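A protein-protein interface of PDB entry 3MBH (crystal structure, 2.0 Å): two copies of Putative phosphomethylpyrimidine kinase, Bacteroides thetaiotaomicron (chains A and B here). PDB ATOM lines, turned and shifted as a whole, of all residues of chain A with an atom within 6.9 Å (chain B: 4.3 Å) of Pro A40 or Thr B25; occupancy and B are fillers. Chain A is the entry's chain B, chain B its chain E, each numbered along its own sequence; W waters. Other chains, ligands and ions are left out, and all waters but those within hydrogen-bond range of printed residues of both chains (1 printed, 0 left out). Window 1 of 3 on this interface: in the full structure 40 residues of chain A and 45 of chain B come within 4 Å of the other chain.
Among the printed residues, pairs that only touch across the chains: Pro A40 with Gly B18 (3.5 Å), Pro A40 with Thr B25 (3.6 Å), Pro A42 with Leu B16 (3.8 Å), Ser A32 with Pro B29 (3.8 Å), Ile A28 with Pro B29 (3.8 Å), Trp A71 with Gly B18 (3.9 Å), Pro A40 with Ser B17 (3.9 Å), Pro A40 with Leu B16 (3.9 Å) and Gln A37 with Gly B20 (3.95 Å).
Positions printed for both chains: 16 and 24.
Of the 10 pairs that touch across the chains among the printed residues, none has its exchanged pair printed and touching as well.
Of the 18 printed residues of chain A, 7 touch a printed residue of chain B.
Hydrophobic or aromatic side chains of chain A that line the printed part of chain B: Ile A28, Pro A40, Pro A42 and Trp A71.
Along chain A the printed residues that touch a printed residue of chain B span positions 28 to 71.
Of the 11 printed residues of chain B, 6 touch a printed residue of chain A.
Hydrophobic or aromatic side chains of chain B within 4 Å of the printed part of chain A: Leu B16 and Pro B29.
Along chain B the printed residues that touch a printed residue of chain A span positions 16 to 29.
Among the printed residues, 10 pairs touch across the chains.
Among the printed residues, no Asp or Glu carboxylate lies within 4 Å of a Lys or Arg side-chain nitrogen of the other chain.
Thr B25 touches just one residue of chain A: Pro A40.
Of the printed residues of chain A, Ser B17 touches Pro A40 (3.9 Å).
Printed residues of chain A within 4 Å of Pro B29: Ile A28 (3.8 Å) and Ser A32 (3.8 Å).
Printed residues of chain B within 4 Å of Cys A39: Gly B18.
Printed residues of chain A within 4 Å of Gly B20: Gln A37.
Ile A10 touches none of the printed residues of chain B.
The nearest printed residue of chain B that does not touch Pro A40 is Gly B20 (6.8 Å).
The backbone carbonyl oxygen (O) of Gly B18 lies close to the side-chain sulfur (SG) of Cys A39.
The backbone NH (N) of Ala A12 lies within hydrogen-bond range of the backbone carbonyl oxygen (O) of Cys A39, 3.1 Å away.
The backbone carbonyl oxygen of Gln A37 lies within hydrogen-bond range of the backbone NH of Ile A10 (2.8 Å).
The side-chain hydroxyl of Thr B25 lies within hydrogen-bond range of the backbone carbonyl oxygen of Val B22.
O of Ile A10 lies within hydrogen-bond range of N of Cys A39 (2.8 Å).
The side-chain hydroxyl (OG) of Ser A32 lies within hydrogen-bond range of the backbone carbonyl oxygen (O) of Ile A28.
Water W1 lies within hydrogen-bond range of the side-chain amide nitrogen (NE2) of Gln A37 (2.9 Å) and the backbone NH (N) of Gly B20 (3.0 Å).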
ATOM      1  N   ILE A  10       4.456 -12.371  24.333  1.00  0.00           N
ATOM      2  CA  ILE A  10       4.199 -12.766  22.986  1.00  0.00           C
ATOM      3  C   ILE A  10       3.457 -11.666  22.246  1.00  0.00           C
ATOM      4  O   ILE A  10       2.335 -11.280  22.634  1.00  0.00           O
ATOM      5  CB  ILE A  10       3.341 -14.031  22.948  1.00  0.00           C
ATOM      6  CG1 ILE A  10       4.002 -15.102  23.782  1.00  0.00           C
ATOM      7  CG2 ILE A  10       3.140 -14.491  21.489  1.00  0.00           C
ATOM      8  CD1 ILE A  10       3.165 -16.378  23.920  1.00  0.00           C
ATOM      9  N   ALA A  11       4.041 -11.175  21.149  1.00  0.00           N
ATOM     10  CA  ALA A  11       3.321 -10.300  20.228  1.00  0.00           C
ATOM     11  C   ALA A  11       2.382 -11.137  19.366  1.00  0.00           C
ATOM     12  O   ALA A  11       2.822 -12.023  18.663  1.00  0.00           O
ATOM     13  CB  ALA A  11       4.347  -9.480  19.321  1.00  0.00           C
ATOM     14  N   ALA A  12       1.087 -10.888  19.449  1.00  0.00           N
ATOM     15  CA  ALA A  12       0.092 -11.623  18.711  1.00  0.00           C
ATOM     16  C   ALA A  12      -0.484 -10.764  17.570  1.00  0.00           C
ATOM     17  O   ALA A  12      -1.243  -9.792  17.806  1.00  0.00           O
ATOM     18  CB  ALA A  12      -1.035 -12.054  19.628  1.00  0.00           C
ATOM     19  N   VAL A  13      -0.143 -11.145  16.357  1.00  0.00           N
ATOM     20  CA  VAL A  13      -0.522 -10.397  15.159  1.00  0.00           C
ATOM     21  C   VAL A  13      -1.740 -11.106  14.520  1.00  0.00           C
ATOM     22  O   VAL A  13      -1.627 -11.942  13.599  1.00  0.00           O
ATOM     23  CB  VAL A  13       0.662 -10.192  14.197  1.00  0.00           C
ATOM     24  CG1 VAL A  13       0.309  -9.180  13.062  1.00  0.00           C
ATOM     25  CG2 VAL A  13       1.961  -9.760  14.992  1.00  0.00           C
ATOM     26  N   HIS A  14      -2.905 -10.730  15.053  1.00  0.00           N
ATOM     27  CA  HIS A  14      -4.199 -11.353  14.780  1.00  0.00           C
ATOM     28  C   HIS A  14      -5.251 -10.271  14.826  1.00  0.00           C
ATOM     29  O   HIS A  14      -5.020  -9.212  15.410  1.00  0.00           O
ATOM     30  CB  HIS A  14      -4.583 -12.381  15.869  1.00  0.00           C
ATOM     31  CG  HIS A  14      -3.674 -13.569  15.931  1.00  0.00           C
ATOM     32  ND1 HIS A  14      -3.993 -14.791  15.370  1.00  0.00           N
ATOM     33  CD2 HIS A  14      -2.444 -13.719  16.478  1.00  0.00           C
ATOM     34  CE1 HIS A  14      -2.999 -15.645  15.576  1.00  0.00           C
ATOM     35  NE2 HIS A  14      -2.048 -15.020  16.260  1.00  0.00           N
ATOM     36  N   LEU A  16      -9.088  -8.742  15.974  1.00  0.00           N
ATOM     37  CA  LEU A  16     -10.020  -8.829  17.087  1.00  0.00           C
ATOM     38  C   LEU A  16     -11.421  -8.977  16.520  1.00  0.00           C
ATOM     39  O   LEU A  16     -11.888  -8.085  15.802  1.00  0.00           O
ATOM     40  CB  LEU A  16      -9.951  -7.581  17.952  1.00  0.00           C
ATOM     41  CG  LEU A  16     -10.717  -7.620  19.254  1.00  0.00           C
ATOM     42  CD1 LEU A  16     -10.051  -8.491  20.288  1.00  0.00           C
ATOM     43  CD2 LEU A  16     -10.934  -6.196  19.754  1.00  0.00           C
ATOM     44  N   LEU A  24      -7.686 -13.212  18.226  1.00  0.00           N
ATOM     45  CA  LEU A  24      -7.254 -12.757  19.538  1.00  0.00           C
ATOM     46  C   LEU A  24      -8.115 -13.252  20.702  1.00  0.00           C
ATOM     47  O   LEU A  24      -7.601 -13.459  21.809  1.00  0.00           O
ATOM     48  CB  LEU A  24      -7.118 -11.246  19.581  1.00  0.00           C
ATOM     49  CG  LEU A  24      -5.955 -10.576  18.856  1.00  0.00           C
ATOM     50  CD1 LEU A  24      -6.080  -9.043  18.932  1.00  0.00           C
ATOM     51  CD2 LEU A  24      -4.587 -11.035  19.456  1.00  0.00           C
ATOM     52  N   ILE A  28      -5.502 -14.849  23.271  1.00  0.00           N
ATOM     53  CA  ILE A  28      -5.307 -14.211  24.546  1.00  0.00           C
ATOM     54  C   ILE A  28      -5.636 -15.188  25.708  1.00  0.00           C
ATOM     55  O   ILE A  28      -4.765 -15.484  26.518  1.00  0.00           O
ATOM     56  CB  ILE A  28      -6.033 -12.830  24.669  1.00  0.00           C
ATOM     57  CG1 ILE A  28      -5.422 -11.801  23.702  1.00  0.00           C
ATOM     58  CG2 ILE A  28      -5.974 -12.316  26.103  1.00  0.00           C
ATOM     59  CD1 ILE A  28      -6.239 -10.544  23.482  1.00  0.00           C
ATOM     60  N   SER A  32      -2.423 -16.698  27.913  1.00  0.00           N
ATOM     61  CA  SER A  32      -2.424 -16.186  29.263  1.00  0.00           C
ATOM     62  C   SER A  32      -2.593 -17.318  30.253  1.00  0.00           C
ATOM     63  O   SER A  32      -1.930 -17.339  31.273  1.00  0.00           O
ATOM     64  CB  SER A  32      -3.475 -15.097  29.485  1.00  0.00           C
ATOM     65  OG  SER A  32      -3.422 -14.118  28.453  1.00  0.00           O
ATOM     66  N   GLN A  37       2.255 -13.441  28.726  1.00  0.00           N
ATOM     67  CA  GLN A  37       1.545 -12.215  28.456  1.00  0.00           C
ATOM     68  C   GLN A  37       1.397 -12.116  26.931  1.00  0.00           C
ATOM     69  O   GLN A  37       2.390 -12.253  26.197  1.00  0.00           O
ATOM     70  CB  GLN A  37       2.283 -10.991  28.992  1.00  0.00           C
ATOM     71  CG  GLN A  37       1.525  -9.695  28.659  1.00  0.00           C
ATOM     72  CD  GLN A  37       2.226  -8.450  29.153  1.00  0.00           C
ATOM     73  OE1 GLN A  37       3.352  -8.486  29.654  1.00  0.00           O
ATOM     74  NE2 GLN A  37       1.528  -7.327  29.021  1.00  0.00           N
ATOM     75  N   VAL A  38       0.156 -11.882  26.472  1.00  0.00           N
ATOM     76  CA  VAL A  38      -0.137 -11.665  25.072  1.00  0.00           C
ATOM     77  C   VAL A  38      -0.316 -10.181  24.803  1.00  0.00           C
ATOM     78  O   VAL A  38      -1.157  -9.529  25.425  1.00  0.00           O
ATOM     79  CB  VAL A  38      -1.366 -12.464  24.677  1.00  0.00           C
ATOM     80  CG1 VAL A  38      -1.790 -12.128  23.253  1.00  0.00           C
ATOM     81  CG2 VAL A  38      -1.053 -13.980  24.836  1.00  0.00           C
ATOM     82  N   CYS A  39       0.536  -9.639  23.934  1.00  0.00           N
ATOM     83  CA  CYS A  39       0.503  -8.230  23.527  1.00  0.00           C
ATOM     84  C   CYS A  39      -0.004  -8.097  22.094  1.00  0.00           C
ATOM     85  O   CYS A  39       0.708  -8.386  21.170  1.00  0.00           O
ATOM     86  CB  CYS A  39       1.915  -7.623  23.593  1.00  0.00           C
ATOM     87  SG  CYS A  39       2.606  -7.775  25.221  1.00  0.00           S
ATOM     88  N   PRO A  40      -1.244  -7.617  21.908  1.00  0.00           N
ATOM     89  CA  PRO A  40      -1.844  -7.666  20.595  1.00  0.00           C
ATOM     90  C   PRO A  40      -1.325  -6.566  19.683  1.00  0.00           C
ATOM     91  O   PRO A  40      -1.170  -5.423  20.102  1.00  0.00           O
ATOM     92  CB  PRO A  40      -3.367  -7.491  20.868  1.00  0.00           C
ATOM     93  CG  PRO A  40      -3.460  -6.859  22.203  1.00  0.00           C
ATOM     94  CD  PRO A  40      -2.208  -7.277  22.964  1.00  0.00           C
ATOM     95  N   LEU A  41      -1.054  -6.969  18.456  1.00  0.00           N
ATOM     96  CA  LEU A  41      -0.865  -6.075  17.311  1.00  0.00           C
ATOM     97  C   LEU A  41      -2.059  -6.400  16.397  1.00  0.00           C
ATOM     98  O   LEU A  41      -1.992  -7.305  15.561  1.00  0.00           O
ATOM     99  CB  LEU A  41       0.497  -6.294  16.667  1.00  0.00           C
ATOM    100  CG  LEU A  41       0.837  -5.427  15.447  1.00  0.00           C
ATOM    101  CD1 LEU A  41       0.937  -3.904  15.817  1.00  0.00           C
ATOM    102  CD2 LEU A  41       2.165  -5.897  14.846  1.00  0.00           C
ATOM    103  N   PRO A  42      -3.213  -5.714  16.628  1.00  0.00           N
ATOM    104  CA  PRO A  42      -4.435  -6.067  15.933  1.00  0.00           C
ATOM    105  C   PRO A  42      -4.387  -5.756  14.438  1.00  0.00           C
ATOM    106  O   PRO A  42      -3.938  -4.674  14.011  1.00  0.00           O
ATOM    107  CB  PRO A  42      -5.508  -5.268  16.659  1.00  0.00           C
ATOM    108  CG  PRO A  42      -4.804  -4.064  17.191  1.00  0.00           C
ATOM    109  CD  PRO A  42      -3.395  -4.534  17.494  1.00  0.00           C
ATOM    110  N   ILE A  67       1.655   1.608  15.907  1.00  0.00           N
ATOM    111  CA  ILE A  67       1.791   0.788  17.107  1.00  0.00           C
ATOM    112  C   ILE A  67       3.208   0.280  17.240  1.00  0.00           C
ATOM    113  O   ILE A  67       3.803   0.368  18.322  1.00  0.00           O
ATOM    114  CB  ILE A  67       0.812  -0.401  17.161  1.00  0.00           C
ATOM    115  CG1 ILE A  67      -0.638   0.125  17.165  1.00  0.00           C
ATOM    116  CG2 ILE A  67       1.083  -1.274  18.449  1.00  0.00           C
ATOM    117  CD1 ILE A  67      -1.759  -0.975  17.073  1.00  0.00           C
ATOM    118  N   TRP A  71       6.020   0.844  20.326  1.00  0.00           N
ATOM    119  CA  TRP A  71       6.705  -0.263  20.956  1.00  0.00           C
ATOM    120  C   TRP A  71       8.210  -0.092  20.944  1.00  0.00           C
ATOM    121  O   TRP A  71       8.906  -0.475  21.910  1.00  0.00           O
ATOM    122  CB  TRP A  71       6.294  -1.577  20.293  1.00  0.00           C
ATOM    123  CG  TRP A  71       4.889  -1.967  20.654  1.00  0.00           C
ATOM    124  CD1 TRP A  71       4.037  -1.312  21.522  1.00  0.00           C
ATOM    125  CD2 TRP A  71       4.183  -3.130  20.206  1.00  0.00           C
ATOM    126  NE1 TRP A  71       2.862  -2.014  21.651  1.00  0.00           N
ATOM    127  CE2 TRP A  71       2.909  -3.118  20.840  1.00  0.00           C
ATOM    128  CE3 TRP A  71       4.495  -4.161  19.341  1.00  0.00           C
ATOM    129  CZ2 TRP A  71       1.948  -4.111  20.616  1.00  0.00           C
ATOM    130  CZ3 TRP A  71       3.541  -5.135  19.099  1.00  0.00           C
ATOM    131  CH2 TRP A  71       2.276  -5.113  19.752  1.00  0.00           C
ATOM    132  N   PHE A  78      10.145  -8.934  22.901  1.00  0.00           N
ATOM    133  CA  PHE A  78       9.233 -10.079  22.816  1.00  0.00           C
ATOM    134  C   PHE A  78      10.019 -11.362  22.780  1.00  0.00           C
ATOM    135  O   PHE A  78      11.021 -11.474  22.067  1.00  0.00           O
ATOM    136  CB  PHE A  78       8.306  -9.993  21.591  1.00  0.00           C
ATOM    137  CG  PHE A  78       7.374  -8.793  21.611  1.00  0.00           C
ATOM    138  CD1 PHE A  78       6.278  -8.767  22.452  1.00  0.00           C
ATOM    139  CD2 PHE A  78       7.572  -7.717  20.751  1.00  0.00           C
ATOM    140  CE1 PHE A  78       5.442  -7.682  22.466  1.00  0.00           C
ATOM    141  CE2 PHE A  78       6.718  -6.623  20.759  1.00  0.00           C
ATOM    142  CZ  PHE A  78       5.665  -6.590  21.614  1.00  0.00           C
ATOM    143  N   LEU B  16      -8.668  -1.844  23.390  1.00  0.00           N
ATOM    144  CA  LEU B  16      -7.588  -2.851  23.230  1.00  0.00           C
ATOM    145  C   LEU B  16      -6.233  -2.121  23.204  1.00  0.00           C
ATOM    146  O   LEU B  16      -5.994  -1.303  22.279  1.00  0.00           O
ATOM    147  CB  LEU B  16      -7.749  -3.602  21.919  1.00  0.00           C
ATOM    148  CG  LEU B  16      -6.764  -4.755  21.732  1.00  0.00           C
ATOM    149  CD1 LEU B  16      -7.258  -5.846  22.662  1.00  0.00           C
ATOM    150  CD2 LEU B  16      -6.658  -5.195  20.252  1.00  0.00           C
ATOM    151  N   SER B  17      -5.408  -2.370  24.228  1.00  0.00           N
ATOM    152  CA  SER B  17      -4.115  -1.776  24.333  1.00  0.00           C
ATOM    153  C   SER B  17      -3.051  -2.857  24.175  1.00  0.00           C
ATOM    154  O   SER B  17      -3.093  -3.916  24.803  1.00  0.00           O
ATOM    155  CB  SER B  17      -3.882  -1.095  25.685  1.00  0.00           C
ATOM    156  OG  SER B  17      -4.535   0.145  25.791  1.00  0.00           O
ATOM    157  N   GLY B  18      -2.057  -2.521  23.381  1.00  0.00           N
ATOM    158  CA  GLY B  18      -1.018  -3.468  23.046  1.00  0.00           C
ATOM    159  C   GLY B  18      -0.096  -3.865  24.175  1.00  0.00           C
ATOM    160  O   GLY B  18       0.221  -5.028  24.288  1.00  0.00           O
ATOM    161  N   GLY B  20       0.998  -3.059  28.446  1.00  0.00           N
ATOM    162  CA  GLY B  20       0.424  -2.667  29.704  1.00  0.00           C
ATOM    163  C   GLY B  20      -0.650  -3.684  29.984  1.00  0.00           C
ATOM    164  O   GLY B  20      -1.100  -4.378  29.070  1.00  0.00           O
ATOM    165  N   VAL B  22      -4.130  -3.446  30.935  1.00  0.00           N
ATOM    166  CA  VAL B  22      -5.345  -2.703  31.115  1.00  0.00           C
ATOM    167  C   VAL B  22      -6.412  -3.324  30.211  1.00  0.00           C
ATOM    168  O   VAL B  22      -6.143  -4.144  29.323  1.00  0.00           O
ATOM    169  CB  VAL B  22      -5.165  -1.197  30.723  1.00  0.00           C
ATOM    170  CG1 VAL B  22      -4.141  -0.540  31.587  1.00  0.00           C
ATOM    171  CG2 VAL B  22      -4.826  -1.084  29.195  1.00  0.00           C
ATOM    172  N   SER B  23      -7.601  -2.860  30.446  1.00  0.00           N
ATOM    173  CA  SER B  23      -8.747  -3.019  29.556  1.00  0.00           C
ATOM    174  C   SER B  23      -8.825  -4.455  28.998  1.00  0.00           C
ATOM    175  O   SER B  23      -8.768  -5.415  29.785  1.00  0.00           O
ATOM    176  CB  SER B  23      -8.660  -1.921  28.494  1.00  0.00           C
ATOM    177  OG  SER B  23      -7.403  -1.906  27.811  1.00  0.00           O
ATOM    178  N   LEU B  24      -9.013  -4.621  27.696  1.00  0.00           N
ATOM    179  CA  LEU B  24      -9.381  -5.975  27.151  1.00  0.00           C
ATOM    180  C   LEU B  24      -8.315  -7.007  27.425  1.00  0.00           C
ATOM    181  O   LEU B  24      -8.631  -8.167  27.633  1.00  0.00           O
ATOM    182  CB  LEU B  24      -9.685  -5.978  25.629  1.00  0.00           C
ATOM    183  CG  LEU B  24     -11.003  -5.320  25.284  1.00  0.00           C
ATOM    184  CD1 LEU B  24     -11.127  -5.132  23.722  1.00  0.00           C
ATOM    185  CD2 LEU B  24     -12.265  -6.025  25.859  1.00  0.00           C
ATOM    186  N   THR B  25      -7.052  -6.603  27.515  1.00  0.00           N
ATOM    187  CA  THR B  25      -6.008  -7.590  27.719  1.00  0.00           C
ATOM    188  C   THR B  25      -5.951  -8.052  29.159  1.00  0.00           C
ATOM    189  O   THR B  25      -5.162  -8.922  29.477  1.00  0.00           O
ATOM    190  CB  THR B  25      -4.636  -7.066  27.257  1.00  0.00           C
ATOM    191  OG1 THR B  25      -4.397  -5.792  27.840  1.00  0.00           O
ATOM    192  CG2 THR B  25      -4.561  -6.966  25.725  1.00  0.00           C
ATOM    193  N   VAL B  26      -6.798  -7.492  30.030  1.00  0.00           N
ATOM    194  CA  VAL B  26      -7.014  -7.987  31.419  1.00  0.00           C
ATOM    195  C   VAL B  26      -8.409  -8.629  31.565  1.00  0.00           C
ATOM    196  O   VAL B  26      -8.514  -9.680  32.185  1.00  0.00           O
ATOM    197  CB  VAL B  26      -6.786  -6.800  32.411  1.00  0.00           C
ATOM    198  CG1 VAL B  26      -7.554  -6.886  33.646  1.00  0.00           C
ATOM    199  CG2 VAL B  26      -5.232  -6.698  32.651  1.00  0.00           C
ATOM    200  N   VAL B  27      -9.441  -8.021  30.966  1.00  0.00           N
ATOM    201  CA  VAL B  27     -10.831  -8.517  31.066  1.00  0.00           C
ATOM    202  C   VAL B  27     -10.911  -9.895  30.433  1.00  0.00           C
ATOM    203  O   VAL B  27     -11.459 -10.836  31.032  1.00  0.00           O
ATOM    204  CB  VAL B  27     -11.780  -7.556  30.392  1.00  0.00           C
ATOM    205  CG1 VAL B  27     -13.196  -8.103  30.332  1.00  0.00           C
ATOM    206  CG2 VAL B  27     -11.685  -6.167  31.110  1.00  0.00           C
ATOM    207  N   PRO B  29      -8.503 -12.368  29.678  1.00  0.00           N
ATOM    208  CA  PRO B  29      -7.937 -13.517  30.400  1.00  0.00           C
ATOM    209  C   PRO B  29      -8.607 -13.829  31.725  1.00  0.00           C
ATOM    210  O   PRO B  29      -8.798 -14.985  32.067  1.00  0.00           O
ATOM    211  CB  PRO B  29      -6.462 -13.095  30.678  1.00  0.00           C
ATOM    212  CG  PRO B  29      -6.301 -11.835  30.149  1.00  0.00           C
ATOM    213  CD  PRO B  29      -7.507 -11.337  29.435  1.00  0.00           C
HETATM  214  O   HOH W   1       2.384  -4.886  30.414  1.00  0.00           O
